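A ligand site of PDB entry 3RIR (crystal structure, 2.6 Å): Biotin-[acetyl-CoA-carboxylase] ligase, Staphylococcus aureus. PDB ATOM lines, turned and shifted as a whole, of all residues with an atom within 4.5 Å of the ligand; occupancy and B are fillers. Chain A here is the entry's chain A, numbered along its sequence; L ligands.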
ATOM      1  N   SER A  93     -29.156  13.639   8.307  1.00  0.00           N
ATOM      2  CA  SER A  93     -27.949  14.402   8.619  1.00  0.00           C
ATOM      3  C   SER A  93     -27.667  14.330  10.087  1.00  0.00           C
ATOM      4  O   SER A  93     -28.579  14.439  10.888  1.00  0.00           O
ATOM      5  CB  SER A  93     -28.073  15.851   8.141  1.00  0.00           C
ATOM      6  OG  SER A  93     -27.287  16.683   8.926  1.00  0.00           O
ATOM      7  N   THR A  94     -26.407  14.132  10.456  1.00  0.00           N
ATOM      8  CA  THR A  94     -26.075  14.221  11.887  1.00  0.00           C
ATOM      9  C   THR A  94     -26.377  15.595  12.531  1.00  0.00           C
ATOM     10  O   THR A  94     -26.659  15.633  13.690  1.00  0.00           O
ATOM     11  CB  THR A  94     -24.608  13.811  12.189  1.00  0.00           C
ATOM     12  OG1 THR A  94     -23.694  14.780  11.684  1.00  0.00           O
ATOM     13  CG2 THR A  94     -24.277  12.501  11.567  1.00  0.00           C
ATOM     14  N   GLN A  95     -26.307  16.718  11.783  1.00  0.00           N
ATOM     15  CA  GLN A  95     -26.668  18.039  12.329  1.00  0.00           C
ATOM     16  C   GLN A  95     -28.133  18.117  12.594  1.00  0.00           C
ATOM     17  O   GLN A  95     -28.522  18.691  13.611  1.00  0.00           O
ATOM     18  CB  GLN A  95     -26.196  19.267  11.468  1.00  0.00           C
ATOM     19  CG  GLN A  95     -24.731  19.513  11.715  1.00  0.00           C
ATOM     20  CD  GLN A  95     -24.451  20.638  12.635  1.00  0.00           C
ATOM     21  OE1 GLN A  95     -23.834  20.490  13.653  1.00  0.00           O
ATOM     22  NE2 GLN A  95     -24.849  21.806  12.253  1.00  0.00           N
ATOM     23  N   GLN A 116     -24.861   9.900   5.208  1.00  0.00           N
ATOM     24  CA  GLN A 116     -25.913  10.882   5.357  1.00  0.00           C
ATOM     25  C   GLN A 116     -26.590  10.962   3.998  1.00  0.00           C
ATOM     26  O   GLN A 116     -25.948  10.927   2.968  1.00  0.00           O
ATOM     27  CB  GLN A 116     -25.346  12.283   5.746  1.00  0.00           C
ATOM     28  CG  GLN A 116     -24.477  12.287   7.000  1.00  0.00           C
ATOM     29  CD  GLN A 116     -24.146  13.657   7.507  1.00  0.00           C
ATOM     30  OE1 GLN A 116     -24.536  14.061   8.639  1.00  0.00           O
ATOM     31  NE2 GLN A 116     -23.385  14.390   6.720  1.00  0.00           N
ATOM     32  N   LYS A 118     -28.887  13.519   3.445  1.00  0.00           N
ATOM     33  CA  LYS A 118     -29.137  14.956   3.200  1.00  0.00           C
ATOM     34  C   LYS A 118     -28.053  15.744   3.923  1.00  0.00           C
ATOM     35  O   LYS A 118     -28.333  16.599   4.769  1.00  0.00           O
ATOM     36  CB  LYS A 118     -30.533  15.384   3.672  1.00  0.00           C
ATOM     37  CG  LYS A 118     -31.035  16.733   3.095  1.00  0.00           C
ATOM     38  CD  LYS A 118     -32.463  17.097   3.608  1.00  0.00           C
ATOM     39  CE  LYS A 118     -33.331  18.017   2.672  1.00  0.00           C
ATOM     40  NZ  LYS A 118     -34.857  18.063   2.923  1.00  0.00           N
ATOM     41  N   GLY A 119     -26.814  15.372   3.633  1.00  0.00           N
ATOM     42  CA  GLY A 119     -25.648  16.069   4.179  1.00  0.00           C
ATOM     43  C   GLY A 119     -25.659  17.503   3.725  1.00  0.00           C
ATOM     44  O   GLY A 119     -25.886  17.788   2.576  1.00  0.00           O
ATOM     45  N   ARG A 120     -25.455  18.452   4.628  1.00  0.00           N
ATOM     46  CA  ARG A 120     -25.404  19.847   4.206  1.00  0.00           C
ATOM     47  C   ARG A 120     -24.237  20.637   4.755  1.00  0.00           C
ATOM     48  O   ARG A 120     -23.862  20.483   5.918  1.00  0.00           O
ATOM     49  CB  ARG A 120     -26.712  20.509   4.550  1.00  0.00           C
ATOM     50  CG  ARG A 120     -27.921  19.970   3.711  1.00  0.00           C
ATOM     51  CD  ARG A 120     -28.038  20.702   2.362  1.00  0.00           C
ATOM     52  NE  ARG A 120     -29.177  20.295   1.562  1.00  0.00           N
ATOM     53  CZ  ARG A 120     -29.311  19.087   1.004  1.00  0.00           C
ATOM     54  NH1 ARG A 120     -28.405  18.126   1.190  1.00  0.00           N
ATOM     55  NH2 ARG A 120     -30.380  18.835   0.277  1.00  0.00           N
ATOM     56  N   GLY A 121     -23.627  21.479   3.919  1.00  0.00           N
ATOM     57  CA  GLY A 121     -22.615  22.369   4.455  1.00  0.00           C
ATOM     58  C   GLY A 121     -23.057  23.799   4.748  1.00  0.00           C
ATOM     59  O   GLY A 121     -24.232  24.110   4.935  1.00  0.00           O
ATOM     60  N   ARG A 122     -22.057  24.666   4.832  1.00  0.00           N
ATOM     61  CA  ARG A 122     -22.234  26.125   4.925  1.00  0.00           C
ATOM     62  C   ARG A 122     -23.136  26.589   3.778  1.00  0.00           C
ATOM     63  O   ARG A 122     -23.119  26.018   2.666  1.00  0.00           O
ATOM     64  CB  ARG A 122     -20.831  26.786   4.964  1.00  0.00           C
ATOM     65  CG  ARG A 122     -20.741  28.137   5.608  1.00  0.00           C
ATOM     66  CD  ARG A 122     -19.593  28.211   6.598  1.00  0.00           C
ATOM     67  NE  ARG A 122     -18.264  28.292   5.998  1.00  0.00           N
ATOM     68  CZ  ARG A 122     -17.754  29.380   5.379  1.00  0.00           C
ATOM     69  NH1 ARG A 122     -18.439  30.517   5.258  1.00  0.00           N
ATOM     70  NH2 ARG A 122     -16.534  29.289   4.871  1.00  0.00           N
ATOM     71  N   PHE A 123     -23.998  27.551   4.078  1.00  0.00           N
ATOM     72  CA  PHE A 123     -24.930  28.133   3.099  1.00  0.00           C
ATOM     73  C   PHE A 123     -25.870  27.105   2.524  1.00  0.00           C
ATOM     74  O   PHE A 123     -26.518  27.332   1.482  1.00  0.00           O
ATOM     75  CB  PHE A 123     -24.167  28.879   1.969  1.00  0.00           C
ATOM     76  CG  PHE A 123     -23.199  29.962   2.488  1.00  0.00           C
ATOM     77  CD1 PHE A 123     -23.683  31.138   3.009  1.00  0.00           C
ATOM     78  CD2 PHE A 123     -21.830  29.771   2.458  1.00  0.00           C
ATOM     79  CE1 PHE A 123     -22.793  32.128   3.537  1.00  0.00           C
ATOM     80  CE2 PHE A 123     -20.936  30.747   2.965  1.00  0.00           C
ATOM     81  CZ  PHE A 123     -21.411  31.904   3.510  1.00  0.00           C
ATOM     82  N   ARG A 125     -25.188  24.296   1.199  1.00  0.00           N
ATOM     83  CA  ARG A 125     -24.705  23.512   0.085  1.00  0.00           C
ATOM     84  C   ARG A 125     -24.750  22.026   0.326  1.00  0.00           C
ATOM     85  O   ARG A 125     -24.688  21.563   1.474  1.00  0.00           O
ATOM     86  CB  ARG A 125     -23.262  23.839  -0.169  1.00  0.00           C
ATOM     87  CG  ARG A 125     -23.067  25.245  -0.785  1.00  0.00           C
ATOM     88  CD  ARG A 125     -21.678  25.596  -0.497  1.00  0.00           C
ATOM     89  NE  ARG A 125     -21.480  27.002  -0.555  1.00  0.00           N
ATOM     90  CZ  ARG A 125     -20.430  27.582  -0.012  1.00  0.00           C
ATOM     91  NH1 ARG A 125     -19.564  26.829   0.623  1.00  0.00           N
ATOM     92  NH2 ARG A 125     -20.254  28.873  -0.117  1.00  0.00           N
ATOM     93  N   HIS A 126     -24.801  21.273  -0.773  1.00  0.00           N
ATOM     94  CA  HIS A 126     -24.821  19.814  -0.722  1.00  0.00           C
ATOM     95  C   HIS A 126     -23.471  19.360  -0.105  1.00  0.00           C
ATOM     96  O   HIS A 126     -22.404  19.870  -0.451  1.00  0.00           O
ATOM     97  CB  HIS A 126     -25.071  19.235  -2.137  1.00  0.00           C
ATOM     98  CG  HIS A 126     -24.883  17.757  -2.221  1.00  0.00           C
ATOM     99  ND1 HIS A 126     -25.906  16.865  -1.928  1.00  0.00           N
ATOM    100  CD2 HIS A 126     -23.803  17.000  -2.528  1.00  0.00           C
ATOM    101  CE1 HIS A 126     -25.447  15.631  -2.036  1.00  0.00           C
ATOM    102  NE2 HIS A 126     -24.168  15.686  -2.392  1.00  0.00           N
ATOM    103  N   TRP A 127     -23.519  18.417   0.830  1.00  0.00           N
ATOM    104  CA  TRP A 127     -22.284  17.840   1.315  1.00  0.00           C
ATOM    105  C   TRP A 127     -22.357  16.330   1.103  1.00  0.00           C
ATOM    106  O   TRP A 127     -23.102  15.650   1.790  1.00  0.00           O
ATOM    107  CB  TRP A 127     -22.000  18.182   2.783  1.00  0.00           C
ATOM    108  CG  TRP A 127     -20.789  17.501   3.263  1.00  0.00           C
ATOM    109  CD1 TRP A 127     -20.725  16.264   3.843  1.00  0.00           C
ATOM    110  CD2 TRP A 127     -19.443  17.965   3.189  1.00  0.00           C
ATOM    111  NE1 TRP A 127     -19.438  15.933   4.152  1.00  0.00           N
ATOM    112  CE2 TRP A 127     -18.614  16.966   3.766  1.00  0.00           C
ATOM    113  CE3 TRP A 127     -18.839  19.142   2.700  1.00  0.00           C
ATOM    114  CZ2 TRP A 127     -17.207  17.067   3.813  1.00  0.00           C
ATOM    115  CZ3 TRP A 127     -17.424  19.271   2.803  1.00  0.00           C
ATOM    116  CH2 TRP A 127     -16.637  18.240   3.355  1.00  0.00           C
ATOM    117  N   SER A 128     -21.536  15.858   0.165  1.00  0.00           N
ATOM    118  CA  SER A 128     -21.428  14.430  -0.197  1.00  0.00           C
ATOM    119  C   SER A 128     -20.866  13.588   0.971  1.00  0.00           C
ATOM    120  O   SER A 128     -19.727  13.819   1.422  1.00  0.00           O
ATOM    121  CB  SER A 128     -20.534  14.255  -1.426  1.00  0.00           C
ATOM    122  OG  SER A 128     -20.607  12.948  -1.964  1.00  0.00           O
ATOM    123  N   TRP A 136     -18.575  11.466   9.461  1.00  0.00           N
ATOM    124  CA  TRP A 136     -19.658  12.453   9.370  1.00  0.00           C
ATOM    125  C   TRP A 136     -20.233  12.550  10.770  1.00  0.00           C
ATOM    126  O   TRP A 136     -20.937  11.639  11.209  1.00  0.00           O
ATOM    127  CB  TRP A 136     -20.757  12.041   8.368  1.00  0.00           C
ATOM    128  CG  TRP A 136     -20.272  11.344   7.128  1.00  0.00           C
ATOM    129  CD1 TRP A 136     -20.638  10.100   6.696  1.00  0.00           C
ATOM    130  CD2 TRP A 136     -19.316  11.818   6.175  1.00  0.00           C
ATOM    131  NE1 TRP A 136     -19.969   9.769   5.550  1.00  0.00           N
ATOM    132  CE2 TRP A 136     -19.156  10.807   5.198  1.00  0.00           C
ATOM    133  CE3 TRP A 136     -18.579  13.002   6.056  1.00  0.00           C
ATOM    134  CZ2 TRP A 136     -18.316  10.945   4.110  1.00  0.00           C
ATOM    135  CZ3 TRP A 136     -17.721  13.129   4.977  1.00  0.00           C
ATOM    136  CH2 TRP A 136     -17.603  12.097   4.017  1.00  0.00           C
ATOM    137  N   MET A 137     -19.954  13.649  11.455  1.00  0.00           N
ATOM    138  CA  MET A 137     -20.155  13.743  12.887  1.00  0.00           C
ATOM    139  C   MET A 137     -20.691  15.108  13.334  1.00  0.00           C
ATOM    140  O   MET A 137     -20.309  16.165  12.841  1.00  0.00           O
ATOM    141  CB  MET A 137     -18.837  13.460  13.584  1.00  0.00           C
ATOM    142  CG  MET A 137     -18.933  13.376  15.127  1.00  0.00           C
ATOM    143  SD  MET A 137     -17.335  13.019  15.896  1.00  0.00           S
ATOM    144  CE  MET A 137     -16.372  14.478  15.694  1.00  0.00           C
ATOM    145  N   SER A 138     -21.582  15.125  14.307  1.00  0.00           N
ATOM    146  CA  SER A 138     -22.027  16.395  14.808  1.00  0.00           C
ATOM    147  C   SER A 138     -21.668  16.359  16.256  1.00  0.00           C
ATOM    148  O   SER A 138     -21.907  15.358  16.910  1.00  0.00           O
ATOM    149  CB  SER A 138     -23.528  16.610  14.568  1.00  0.00           C
ATOM    150  OG  SER A 138     -23.732  17.124  13.254  1.00  0.00           O
ATOM    151  N   ASP A 180     -12.382  25.307   6.578  1.00  0.00           N
ATOM    152  CA  ASP A 180     -11.937  24.194   5.733  1.00  0.00           C
ATOM    153  C   ASP A 180     -10.581  23.685   6.110  1.00  0.00           C
ATOM    154  O   ASP A 180      -9.780  24.389   6.632  1.00  0.00           O
ATOM    155  CB  ASP A 180     -11.982  24.576   4.291  1.00  0.00           C
ATOM    156  CG  ASP A 180     -13.353  25.024   3.871  1.00  0.00           C
ATOM    157  OD1 ASP A 180     -13.725  24.831   2.719  1.00  0.00           O
ATOM    158  OD2 ASP A 180     -14.059  25.581   4.700  1.00  0.00           O
ATOM    159  N   LYS A 187      -9.432  19.829  -0.480  1.00  0.00           N
ATOM    160  CA  LYS A 187     -10.270  19.994   0.686  1.00  0.00           C
ATOM    161  C   LYS A 187     -10.503  18.602   1.282  1.00  0.00           C
ATOM    162  O   LYS A 187     -11.122  17.763   0.678  1.00  0.00           O
ATOM    163  CB  LYS A 187     -11.589  20.678   0.348  1.00  0.00           C
ATOM    164  CG  LYS A 187     -12.420  20.967   1.587  1.00  0.00           C
ATOM    165  CD  LYS A 187     -13.758  21.543   1.302  1.00  0.00           C
ATOM    166  CE  LYS A 187     -14.475  22.031   2.569  1.00  0.00           C
ATOM    167  NZ  LYS A 187     -15.692  22.861   2.281  1.00  0.00           N
ATOM    168  N   GLY A 190     -14.658  19.820   5.975  1.00  0.00           N
ATOM    169  CA  GLY A 190     -15.365  21.078   6.181  1.00  0.00           C
ATOM    170  C   GLY A 190     -16.056  20.977   7.518  1.00  0.00           C
ATOM    171  O   GLY A 190     -16.594  19.964   7.900  1.00  0.00           O
ATOM    172  N   PHE A 191     -16.044  22.029   8.295  1.00  0.00           N
ATOM    173  CA  PHE A 191     -16.784  21.928   9.525  1.00  0.00           C
ATOM    174  C   PHE A 191     -17.697  23.144   9.590  1.00  0.00           C
ATOM    175  O   PHE A 191     -17.485  24.151   8.918  1.00  0.00           O
ATOM    176  CB  PHE A 191     -15.847  21.760  10.726  1.00  0.00           C
ATOM    177  CG  PHE A 191     -14.880  22.847  10.888  1.00  0.00           C
ATOM    178  CD1 PHE A 191     -13.758  22.950  10.049  1.00  0.00           C
ATOM    179  CD2 PHE A 191     -15.047  23.789  11.889  1.00  0.00           C
ATOM    180  CE1 PHE A 191     -12.843  23.975  10.178  1.00  0.00           C
ATOM    181  CE2 PHE A 191     -14.097  24.827  12.064  1.00  0.00           C
ATOM    182  CZ  PHE A 191     -13.011  24.907  11.200  1.00  0.00           C
ATOM    183  N   LEU A 192     -18.755  23.015  10.353  1.00  0.00           N
ATOM    184  CA  LEU A 192     -19.827  23.954  10.409  1.00  0.00           C
ATOM    185  C   LEU A 192     -20.054  24.133  11.919  1.00  0.00           C
ATOM    186  O   LEU A 192     -20.370  23.168  12.610  1.00  0.00           O
ATOM    187  CB  LEU A 192     -21.047  23.249   9.755  1.00  0.00           C
ATOM    188  CG  LEU A 192     -22.284  24.101   9.563  1.00  0.00           C
ATOM    189  CD1 LEU A 192     -21.876  25.361   8.892  1.00  0.00           C
ATOM    190  CD2 LEU A 192     -23.260  23.426   8.736  1.00  0.00           C
ATOM    191  N   GLY A 208     -20.876  20.514  13.246  1.00  0.00           N
ATOM    192  CA  GLY A 208     -20.825  19.503  12.211  1.00  0.00           C
ATOM    193  C   GLY A 208     -19.487  19.371  11.465  1.00  0.00           C
ATOM    194  O   GLY A 208     -19.062  20.303  10.755  1.00  0.00           O
ATOM    195  N   ILE A 209     -18.879  18.188  11.562  1.00  0.00           N
ATOM    196  CA  ILE A 209     -17.584  17.863  10.984  1.00  0.00           C
ATOM    197  C   ILE A 209     -17.595  16.739   9.939  1.00  0.00           C
ATOM    198  O   ILE A 209     -17.863  15.570  10.239  1.00  0.00           O
ATOM    199  CB  ILE A 209     -16.605  17.447  12.104  1.00  0.00           C
ATOM    200  CG1 ILE A 209     -16.434  18.591  13.086  1.00  0.00           C
ATOM    201  CG2 ILE A 209     -15.284  17.022  11.543  1.00  0.00           C
ATOM    202  CD1 ILE A 209     -15.730  18.215  14.279  1.00  0.00           C
ATOM    203  N   GLY A 210     -17.289  17.079   8.714  1.00  0.00           N
ATOM    204  CA  GLY A 210     -17.154  16.087   7.661  1.00  0.00           C
ATOM    205  C   GLY A 210     -15.699  15.975   7.238  1.00  0.00           C
ATOM    206  O   GLY A 210     -15.094  16.960   6.767  1.00  0.00           O
ATOM    207  N   ASN A 212     -12.961  13.531   5.016  1.00  0.00           N
ATOM    208  CA  ASN A 212     -12.867  12.456   4.040  1.00  0.00           C
ATOM    209  C   ASN A 212     -11.791  11.449   4.439  1.00  0.00           C
ATOM    210  O   ASN A 212     -10.675  11.822   4.666  1.00  0.00           O
ATOM    211  CB  ASN A 212     -12.544  13.015   2.699  1.00  0.00           C
ATOM    212  CG  ASN A 212     -13.658  13.911   2.115  1.00  0.00           C
ATOM    213  OD1 ASN A 212     -14.824  13.671   2.310  1.00  0.00           O
ATOM    214  ND2 ASN A 212     -13.268  14.915   1.332  1.00  0.00           N
ATOM    215  N   PHE A 220     -15.050  11.003  -6.275  1.00  0.00           N
ATOM    216  CA  PHE A 220     -15.577  12.367  -6.220  1.00  0.00           C
ATOM    217  C   PHE A 220     -16.118  12.882  -7.590  1.00  0.00           C
ATOM    218  O   PHE A 220     -15.400  12.799  -8.599  1.00  0.00           O
ATOM    219  CB  PHE A 220     -14.444  13.304  -5.863  1.00  0.00           C
ATOM    220  CG  PHE A 220     -13.804  13.058  -4.514  1.00  0.00           C
ATOM    221  CD1 PHE A 220     -14.434  13.412  -3.357  1.00  0.00           C
ATOM    222  CD2 PHE A 220     -12.514  12.579  -4.420  1.00  0.00           C
ATOM    223  CE1 PHE A 220     -13.834  13.231  -2.117  1.00  0.00           C
ATOM    224  CE2 PHE A 220     -11.918  12.414  -3.196  1.00  0.00           C
ATOM    225  CZ  PHE A 220     -12.584  12.754  -2.035  1.00  0.00           C
ATOM    226  N   ARG A 227     -10.199  19.836  -6.326  1.00  0.00           N
ATOM    227  CA  ARG A 227     -10.022  20.467  -5.031  1.00  0.00           C
ATOM    228  C   ARG A 227     -10.556  19.599  -3.905  1.00  0.00           C
ATOM    229  O   ARG A 227     -10.955  20.096  -2.864  1.00  0.00           O
ATOM    230  CB  ARG A 227     -10.678  21.830  -5.023  1.00  0.00           C
ATOM    231  CG  ARG A 227     -12.071  21.762  -5.513  1.00  0.00           C
ATOM    232  CD  ARG A 227     -12.653  23.122  -5.687  1.00  0.00           C
ATOM    233  NE  ARG A 227     -13.861  23.043  -6.493  1.00  0.00           N
ATOM    234  CZ  ARG A 227     -15.076  22.822  -5.997  1.00  0.00           C
ATOM    235  NH1 ARG A 227     -16.132  22.755  -6.803  1.00  0.00           N
ATOM    236  NH2 ARG A 227     -15.225  22.675  -4.673  1.00  0.00           N
ATOM    237  N   ALA A 228     -10.581  18.285  -4.113  1.00  0.00           N
ATOM    238  CA  ALA A 228     -10.960  17.322  -3.059  1.00  0.00           C
ATOM    239  C   ALA A 228      -9.876  16.235  -2.849  1.00  0.00           C
ATOM    240  O   ALA A 228      -9.131  15.941  -3.764  1.00  0.00           O
ATOM    241  CB  ALA A 228     -12.253  16.674  -3.383  1.00  0.00           C
HETATM  242  C1  LIG L   1     -19.139  22.747   4.754  1.00  0.00           C
HETATM  243  O1  LIG L   1     -19.698  23.838   4.089  1.00  0.00           O
HETATM  244  O2  LIG L   1     -17.988  22.732   4.334  1.00  0.00           O
HETATM  245  C2  LIG L   1     -19.059  21.951   5.887  1.00  0.00           C
HETATM  246  C3  LIG L   1     -19.931  20.920   6.115  1.00  0.00           C
HETATM  247  C4  LIG L   1     -19.593  19.849   7.098  1.00  0.00           C
HETATM  248  C5  LIG L   1     -20.290  18.484   6.953  1.00  0.00           C
HETATM  249  C6  LIG L   1     -20.476  17.736   8.181  1.00  0.00           C
HETATM  250  S1  LIG L   1     -20.846  16.112   7.839  1.00  0.00           S
HETATM  251  C7  LIG L   1     -21.195  15.959   9.506  1.00  0.00           C
HETATM  252  C8  LIG L   1     -22.355  16.870   9.280  1.00  0.00           C
HETATM  253  N1  LIG L   1     -23.566  16.769   9.090  1.00  0.00           N
HETATM  254  C9  LIG L   1     -23.928  17.766   8.265  1.00  0.00           C
HETATM  255  O3  LIG L   1     -25.036  17.670   7.503  1.00  0.00           O
HETATM  256  N2  LIG L   1     -22.845  18.588   7.856  1.00  0.00           N
HETATM  257  C10 LIG L   1     -21.864  17.986   8.535  1.00  0.00           C
HETATM  258  P1  LIG L   1     -19.559  24.460   2.625  1.00  0.00           P
HETATM  259  O4  LIG L   1     -18.175  25.105   2.469  1.00  0.00           O
HETATM  260  O5  LIG L   1     -20.760  25.341   2.623  1.00  0.00           O
HETATM  261  O6  LIG L   1     -19.760  23.316   1.525  1.00  0.00           O
HETATM  262  C11 LIG L   1     -18.737  22.406   1.225  1.00  0.00           C
HETATM  263  C12 LIG L   1     -18.148  22.678  -0.114  1.00  0.00           C
HETATM  264  O7  LIG L   1     -17.463  21.491  -0.563  1.00  0.00           O
HETATM  265  C13 LIG L   1     -19.160  22.984  -1.211  1.00  0.00           C
HETATM  266  O8  LIG L   1     -18.480  23.593  -2.325  1.00  0.00           O
HETATM  267  C14 LIG L   1     -19.572  21.592  -1.628  1.00  0.00           C
HETATM  268  O9  LIG L   1     -20.184  21.533  -2.900  1.00  0.00           O
HETATM  269  C15 LIG L   1     -18.207  20.891  -1.612  1.00  0.00           C
HETATM  270  N3  LIG L   1     -18.272  19.463  -1.333  1.00  0.00           N
HETATM  271  C16 LIG L   1     -19.290  18.610  -1.164  1.00  0.00           C
HETATM  272  N4  LIG L   1     -18.769  17.478  -0.680  1.00  0.00           N
HETATM  273  C17 LIG L   1     -17.400  17.635  -0.550  1.00  0.00           C
HETATM  274  C18 LIG L   1     -16.351  16.798  -0.099  1.00  0.00           C
HETATM  275  N5  LIG L   1     -16.682  15.438   0.345  1.00  0.00           N
HETATM  276  N6  LIG L   1     -15.061  17.305  -0.084  1.00  0.00           N
HETATM  277  C19 LIG L   1     -14.781  18.567  -0.502  1.00  0.00           C
HETATM  278  N7  LIG L   1     -15.772  19.367  -0.928  1.00  0.00           N
HETATM  279  C20 LIG L   1     -17.084  18.931  -0.950  1.00  0.00           C
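The backbone NH (N) of Arg 122 sits at hydrogen-bond distance from an oxygen (O1) of the ligand (2.6 Å). An oxygen (O5) of the ligand sits close to the backbone carbonyl oxygen of Arg 122, 2.5 Å away. The guanidinium group (NH1) of Arg 125 lies within salt-bridge range of an oxygen (O5) of the ligand. An oxygen (O3) of the ligand sits at hydrogen-bond distance from the side-chain hydroxyl (OG) of Ser 93, 2.8 Å away. An oxygen (O3) of the ligand sits at hydrogen-bond distance from the backbone NH (N) of Arg 120 (3.0 Å). The backbone carbonyl oxygen of Arg 120 lies within hydrogen-bond range of a nitrogen (N2) of the ligand. OE1 of Gln 116 sits at hydrogen-bond distance from N1 of the ligand (2.9 Å). O4 of the ligand lies within salt-bridge range of NZ of Lys 187. OD1 of Asn 212 sits at hydrogen-bond distance from N5 of the ligand, at 3.2 Å. A nitrogen (N1) of the ligand lies within hydrogen-bond range of the side-chain hydroxyl (OG1) of Thr 94 (3.3 Å). S1 of the ligand sits close to N of Gly 210, at 3.8 Å. A nitrogen (N4) of the ligand lies within hydrogen-bond range of the backbone NH (N) of Ser 128 (3.3 Å).
OG of Ser 93 lies within hydrogen-bond range of N of Gln 95 (3.0 Å). OE1 of Gln 116 lies within hydrogen-bond range of N of Thr 94 (2.6 Å). The backbone NH (N) of Lys 187 is in hydrogen-bond range of the backbone carbonyl oxygen (O) of Arg 227 (2.8 Å). NZ of Lys 187 is in salt-bridge range of OD1 of Asp 180 (2.8 Å). OG of Ser 138 sits at hydrogen-bond distance from OG1 of Thr 94 (2.8 Å). The side-chain amide oxygen of Gln 95 lies within hydrogen-bond range of the backbone NH of Gly 208, 3.0 Å away. N of Leu 192 is in hydrogen-bond range of O of Gly 208, 2.8 Å away. OG of Ser 138 is in hydrogen-bond range of N of Gln 95.
N of Gln 95 touches N1 of the ligand, at 3.8 Å. Gly 119 touches the ligand. Gly 121 touches the ligand. His 126 touches the ligand. Trp 127 touches the ligand. Trp 136 touches the ligand (C to C7, 3.8 Å). Met 137 touches the ligand. Gly 190 touches the ligand. Phe 191 touches the ligand (N to C2, 3.9 Å). Gly 208 touches the ligand. Ile 209 touches the ligand. Hydrophobic or aromatic side chains within 4 Å of the ligand: Trp 127. Of the 29 residues printed, 21 come within 4 Å of the ligand. The nearest printed residue that does not touch the ligand is Arg 227 (4.1 Å).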
